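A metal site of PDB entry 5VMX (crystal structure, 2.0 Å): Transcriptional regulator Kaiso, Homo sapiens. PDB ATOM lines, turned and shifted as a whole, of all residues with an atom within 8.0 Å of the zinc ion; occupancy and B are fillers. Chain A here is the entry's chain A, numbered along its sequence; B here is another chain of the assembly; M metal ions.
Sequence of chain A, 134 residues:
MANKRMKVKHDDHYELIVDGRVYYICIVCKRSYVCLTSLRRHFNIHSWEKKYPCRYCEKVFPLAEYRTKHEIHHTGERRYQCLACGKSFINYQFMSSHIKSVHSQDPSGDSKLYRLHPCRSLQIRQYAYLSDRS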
ATOM      1  N   ASP A  12     -24.427  32.371  19.830  1.00  0.00           N
ATOM      2  CA  ASP A  12     -25.374  31.280  19.829  1.00  0.00           C
ATOM      3  C   ASP A  12     -24.584  29.978  19.747  1.00  0.00           C
ATOM      4  O   ASP A  12     -25.121  28.919  19.391  1.00  0.00           O
ATOM      5  CB  ASP A  12     -26.333  31.405  18.643  1.00  0.00           C
ATOM      6  CG  ASP A  12     -25.608  31.633  17.335  1.00  0.00           C
ATOM      7  OD1 ASP A  12     -24.349  31.652  17.346  1.00  0.00           O
ATOM      8  OD2 ASP A  12     -26.279  31.787  16.293  1.00  0.00           O
ATOM      9  N   ILE A  25     -19.779  24.917  18.177  1.00  0.00           N
ATOM     10  CA  ILE A  25     -20.757  24.076  18.850  1.00  0.00           C
ATOM     11  C   ILE A  25     -22.029  24.860  19.134  1.00  0.00           C
ATOM     12  O   ILE A  25     -21.990  25.917  19.781  1.00  0.00           O
ATOM     13  CB  ILE A  25     -20.212  23.495  20.198  1.00  0.00           C
ATOM     14  CG1 ILE A  25     -19.266  22.331  19.962  1.00  0.00           C
ATOM     15  CG2 ILE A  25     -21.356  22.959  21.023  1.00  0.00           C
ATOM     16  CD1 ILE A  25     -17.970  22.688  19.317  1.00  0.00           C
ATOM     17  N   CYS A  26     -23.152  24.330  18.666  1.00  0.00           N
ATOM     18  CA  CYS A  26     -24.454  24.976  18.865  1.00  0.00           C
ATOM     19  C   CYS A  26     -24.857  24.942  20.329  1.00  0.00           C
ATOM     20  O   CYS A  26     -24.907  23.878  20.939  1.00  0.00           O
ATOM     21  CB  CYS A  26     -25.512  24.275  18.016  1.00  0.00           C
ATOM     22  SG  CYS A  26     -27.172  24.897  18.301  1.00  0.00           S
ATOM     23  N   ILE A  27     -25.161  26.111  20.889  1.00  0.00           N
ATOM     24  CA  ILE A  27     -25.384  26.196  22.336  1.00  0.00           C
ATOM     25  C   ILE A  27     -26.693  25.513  22.744  1.00  0.00           C
ATOM     26  O   ILE A  27     -26.867  25.140  23.891  1.00  0.00           O
ATOM     27  CB  ILE A  27     -25.383  27.667  22.833  1.00  0.00           C
ATOM     28  CG1 ILE A  27     -25.252  27.726  24.351  1.00  0.00           C
ATOM     29  CG2 ILE A  27     -26.620  28.403  22.367  1.00  0.00           C
ATOM     30  CD1 ILE A  27     -24.224  26.772  24.925  1.00  0.00           C
ATOM     31  N   VAL A  28     -27.595  25.311  21.788  1.00  0.00           N
ATOM     32  CA  VAL A  28     -28.882  24.689  22.107  1.00  0.00           C
ATOM     33  C   VAL A  28     -28.815  23.156  22.071  1.00  0.00           C
ATOM     34  O   VAL A  28     -29.040  22.509  23.090  1.00  0.00           O
ATOM     35  CB  VAL A  28     -29.977  25.171  21.157  1.00  0.00           C
ATOM     36  CG1 VAL A  28     -31.255  24.365  21.369  1.00  0.00           C
ATOM     37  CG2 VAL A  28     -30.238  26.656  21.370  1.00  0.00           C
ATOM     38  N   CYS A  29     -28.508  22.576  20.909  1.00  0.00           N
ATOM     39  CA  CYS A  29     -28.497  21.111  20.777  1.00  0.00           C
ATOM     40  C   CYS A  29     -27.104  20.478  20.847  1.00  0.00           C
ATOM     41  O   CYS A  29     -26.989  19.255  20.845  1.00  0.00           O
ATOM     42  CB  CYS A  29     -29.167  20.693  19.471  1.00  0.00           C
ATOM     43  SG  CYS A  29     -28.294  21.200  17.963  1.00  0.00           S
ATOM     44  N   LYS A  30     -26.066  21.310  20.896  1.00  0.00           N
ATOM     45  CA  LYS A  30     -24.662  20.879  20.954  1.00  0.00           C
ATOM     46  C   LYS A  30     -24.156  20.154  19.697  1.00  0.00           C
ATOM     47  O   LYS A  30     -23.199  19.380  19.757  1.00  0.00           O
ATOM     48  CB  LYS A  30     -24.427  19.967  22.179  1.00  0.00           C
ATOM     49  CG  LYS A  30     -24.838  20.594  23.516  1.00  0.00           C
ATOM     50  CD  LYS A  30     -23.897  21.710  23.937  1.00  0.00           C
ATOM     51  CE  LYS A  30     -24.115  22.092  25.403  1.00  0.00           C
ATOM     52  NZ  LYS A  30     -25.505  22.563  25.667  1.00  0.00           N
ATOM     53  N   ARG A  31     -24.762  20.417  18.540  1.00  0.00           N
ATOM     54  CA  ARG A  31     -24.210  19.869  17.308  1.00  0.00           C
ATOM     55  C   ARG A  31     -22.916  20.601  16.990  1.00  0.00           C
ATOM     56  O   ARG A  31     -22.787  21.784  17.334  1.00  0.00           O
ATOM     57  CB  ARG A  31     -25.196  19.994  16.131  1.00  0.00           C
ATOM     58  CG  ARG A  31     -26.234  18.882  16.102  1.00  0.00           C
ATOM     59  CD  ARG A  31     -27.244  19.093  14.987  1.00  0.00           C
ATOM     60  NE  ARG A  31     -28.290  18.072  14.980  1.00  0.00           N
ATOM     61  CZ  ARG A  31     -28.264  16.996  14.196  1.00  0.00           C
ATOM     62  NH1 ARG A  31     -27.247  16.799  13.367  1.00  0.00           N
ATOM     63  NH2 ARG A  31     -29.255  16.116  14.242  1.00  0.00           N
ATOM     64  N   SER A  32     -21.953  19.931  16.369  1.00  0.00           N
ATOM     65  CA  SER A  32     -20.682  20.582  16.026  1.00  0.00           C
ATOM     66  C   SER A  32     -20.535  20.844  14.536  1.00  0.00           C
ATOM     67  O   SER A  32     -21.017  20.083  13.691  1.00  0.00           O
ATOM     68  CB  SER A  32     -19.491  19.764  16.530  1.00  0.00           C
ATOM     69  OG  SER A  32     -19.366  18.535  15.839  1.00  0.00           O
ATOM     70  N   TYR A  33     -19.863  21.940  14.216  1.00  0.00           N
ATOM     71  CA  TYR A  33     -19.694  22.417  12.858  1.00  0.00           C
ATOM     72  C   TYR A  33     -18.262  22.820  12.612  1.00  0.00           C
ATOM     73  O   TYR A  33     -17.610  23.424  13.472  1.00  0.00           O
ATOM     74  CB  TYR A  33     -20.650  23.590  12.606  1.00  0.00           C
ATOM     75  CG  TYR A  33     -22.073  23.121  12.724  1.00  0.00           C
ATOM     76  CD1 TYR A  33     -22.737  23.170  13.950  1.00  0.00           C
ATOM     77  CD2 TYR A  33     -22.719  22.531  11.640  1.00  0.00           C
ATOM     78  CE1 TYR A  33     -24.032  22.691  14.071  1.00  0.00           C
ATOM     79  CE2 TYR A  33     -24.004  22.050  11.747  1.00  0.00           C
ATOM     80  CZ  TYR A  33     -24.655  22.142  12.969  1.00  0.00           C
ATOM     81  OH  TYR A  33     -25.938  21.647  13.079  1.00  0.00           O
ATOM     82  N   LEU A  39     -23.089  26.567  11.180  1.00  0.00           N
ATOM     83  CA  LEU A  39     -23.776  26.690  12.449  1.00  0.00           C
ATOM     84  C   LEU A  39     -24.867  27.752  12.327  1.00  0.00           C
ATOM     85  O   LEU A  39     -25.978  27.548  12.814  1.00  0.00           O
ATOM     86  CB  LEU A  39     -22.820  27.048  13.586  1.00  0.00           C
ATOM     87  CG  LEU A  39     -23.539  27.233  14.915  1.00  0.00           C
ATOM     88  CD1 LEU A  39     -22.802  26.475  15.994  1.00  0.00           C
ATOM     89  CD2 LEU A  39     -23.632  28.721  15.266  1.00  0.00           C
ATOM     90  N   HIS A  42     -27.755  26.298  10.427  1.00  0.00           N
ATOM     91  CA  HIS A  42     -28.458  25.364  11.292  1.00  0.00           C
ATOM     92  C   HIS A  42     -29.310  26.030  12.389  1.00  0.00           C
ATOM     93  O   HIS A  42     -30.414  25.575  12.700  1.00  0.00           O
ATOM     94  CB  HIS A  42     -27.434  24.413  11.942  1.00  0.00           C
ATOM     95  CG  HIS A  42     -27.925  23.793  13.208  1.00  0.00           C
ATOM     96  ND1 HIS A  42     -28.798  22.735  13.227  1.00  0.00           N
ATOM     97  CD2 HIS A  42     -27.657  24.094  14.497  1.00  0.00           C
ATOM     98  CE1 HIS A  42     -29.063  22.401  14.482  1.00  0.00           C
ATOM     99  NE2 HIS A  42     -28.378  23.209  15.268  1.00  0.00           N
ATOM    100  N   PHE A  43     -28.816  27.124  12.968  1.00  0.00           N
ATOM    101  CA  PHE A  43     -29.408  27.673  14.192  1.00  0.00           C
ATOM    102  C   PHE A  43     -30.811  28.255  13.963  1.00  0.00           C
ATOM    103  O   PHE A  43     -31.629  28.389  14.893  1.00  0.00           O
ATOM    104  CB  PHE A  43     -28.495  28.758  14.772  1.00  0.00           C
ATOM    105  CG  PHE A  43     -28.826  29.141  16.189  1.00  0.00           C
ATOM    106  CD1 PHE A  43     -28.469  28.332  17.247  1.00  0.00           C
ATOM    107  CD2 PHE A  43     -29.506  30.321  16.461  1.00  0.00           C
ATOM    108  CE1 PHE A  43     -28.773  28.682  18.544  1.00  0.00           C
ATOM    109  CE2 PHE A  43     -29.811  30.685  17.755  1.00  0.00           C
ATOM    110  CZ  PHE A  43     -29.443  29.860  18.803  1.00  0.00           C
ATOM    111  N   ASN A  44     -31.107  28.578  12.707  1.00  0.00           N
ATOM    112  CA  ASN A  44     -32.425  29.072  12.353  1.00  0.00           C
ATOM    113  C   ASN A  44     -33.509  28.064  12.693  1.00  0.00           C
ATOM    114  O   ASN A  44     -34.641  28.441  12.991  1.00  0.00           O
ATOM    115  CB  ASN A  44     -32.505  29.413  10.876  1.00  0.00           C
ATOM    116  CG  ASN A  44     -33.610  30.404  10.581  1.00  0.00           C
ATOM    117  OD1 ASN A  44     -33.751  31.410  11.291  1.00  0.00           O
ATOM    118  ND2 ASN A  44     -34.432  30.116   9.576  1.00  0.00           N
ATOM    119  N   ILE A  45     -33.156  26.790  12.665  1.00  0.00           N
ATOM    120  CA  ILE A  45     -34.051  25.710  13.101  1.00  0.00           C
ATOM    121  C   ILE A  45     -34.514  25.907  14.546  1.00  0.00           C
ATOM    122  O   ILE A  45     -35.662  25.635  14.879  1.00  0.00           O
ATOM    123  CB  ILE A  45     -33.359  24.341  12.950  1.00  0.00           C
ATOM    124  CG1 ILE A  45     -33.020  24.104  11.470  1.00  0.00           C
ATOM    125  CG2 ILE A  45     -34.237  23.226  13.476  1.00  0.00           C
ATOM    126  CD1 ILE A  45     -32.059  22.956  11.235  1.00  0.00           C
ATOM    127  N   HIS A  46     -33.616  26.407  15.404  1.00  0.00           N
ATOM    128  CA  HIS A  46     -33.966  26.700  16.786  1.00  0.00           C
ATOM    129  C   HIS A  46     -34.689  28.039  16.912  1.00  0.00           C
ATOM    130  O   HIS A  46     -35.724  28.131  17.578  1.00  0.00           O
ATOM    131  CB  HIS A  46     -32.724  26.714  17.686  1.00  0.00           C
ATOM    132  CG  HIS A  46     -31.968  25.427  17.678  1.00  0.00           C
ATOM    133  ND1 HIS A  46     -32.576  24.197  17.836  1.00  0.00           N
ATOM    134  CD2 HIS A  46     -30.639  25.172  17.519  1.00  0.00           C
ATOM    135  CE1 HIS A  46     -31.664  23.241  17.786  1.00  0.00           C
ATOM    136  NE2 HIS A  46     -30.480  23.813  17.602  1.00  0.00           N
ATOM    137  N1  5CM B   8     -24.391  20.099   5.423  1.00  0.00           N
ATOM    138  C2  5CM B   8     -24.229  19.409   4.122  1.00  0.00           C
ATOM    139  N3  5CM B   8     -25.291  19.523   3.116  1.00  0.00           N
ATOM    140  C4  5CM B   8     -26.492  20.253   3.390  1.00  0.00           C
ATOM    141  C5  5CM B   8     -26.668  20.944   4.695  1.00  0.00           C
ATOM    142  C5A 5CM B   8     -27.929  21.753   4.991  1.00  0.00           C
ATOM    143  C6  5CM B   8     -25.598  20.852   5.704  1.00  0.00           C
ATOM    144  O2  5CM B   8     -23.238  18.790   3.869  1.00  0.00           O
ATOM    145  N4  5CM B   8     -27.485  20.299   2.345  1.00  0.00           N
ATOM    146  C1' 5CM B   8     -23.295  19.938   6.375  1.00  0.00           C
ATOM    147  C2' 5CM B   8     -23.232  20.982   7.550  1.00  0.00           C
ATOM    148  C3' 5CM B   8     -22.277  20.223   8.457  1.00  0.00           C
ATOM    149  C4' 5CM B   8     -22.661  18.921   8.351  1.00  0.00           C
ATOM    150  O4' 5CM B   8     -23.511  18.816   6.982  1.00  0.00           O
ATOM    151  O3' 5CM B   8     -20.935  20.335   7.838  1.00  0.00           O
ATOM    152  C5' 5CM B   8     -23.517  18.454   9.495  1.00  0.00           C
ATOM    153  O5' 5CM B   8     -24.597  19.338   9.665  1.00  0.00           O
ATOM    154  P   5CM B   8     -25.800  18.907  10.711  1.00  0.00           P
ATOM    155  OP1 5CM B   8     -25.210  18.268  11.950  1.00  0.00           O
ATOM    156  OP2 5CM B   8     -26.691  20.093  11.021  1.00  0.00           O
HETATM  157 ZN    ZN M   1     -28.592  23.312  17.349  1.00  0.00          ZN
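OH of Tyr 33 sits close to ND1 of His 42 (3.1 Å). The side-chain sulfur (SG) of Cys 29 lies close to the backbone NH (N) of Arg 31, 3.7 Å away. The backbone NH of Val 28 sits close to the side-chain sulfur of Cys 26 (3.5 Å). The backbone carbonyl oxygen (O) of Arg 31 is in hydrogen-bond range of the backbone NH (N) of Cys 26 (2.9 Å).
The zinc ion is bound by a ring nitrogen (NE2) of His 46 (2.0 Å), a ring nitrogen (NE2) of His 42 (2.1 Å), the side-chain sulfur (SG) of Cys 29 (2.2 Å) and the side-chain sulfur (SG) of Cys 26 (2.3 Å). The zinc ion has four donor atoms within binding distance.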
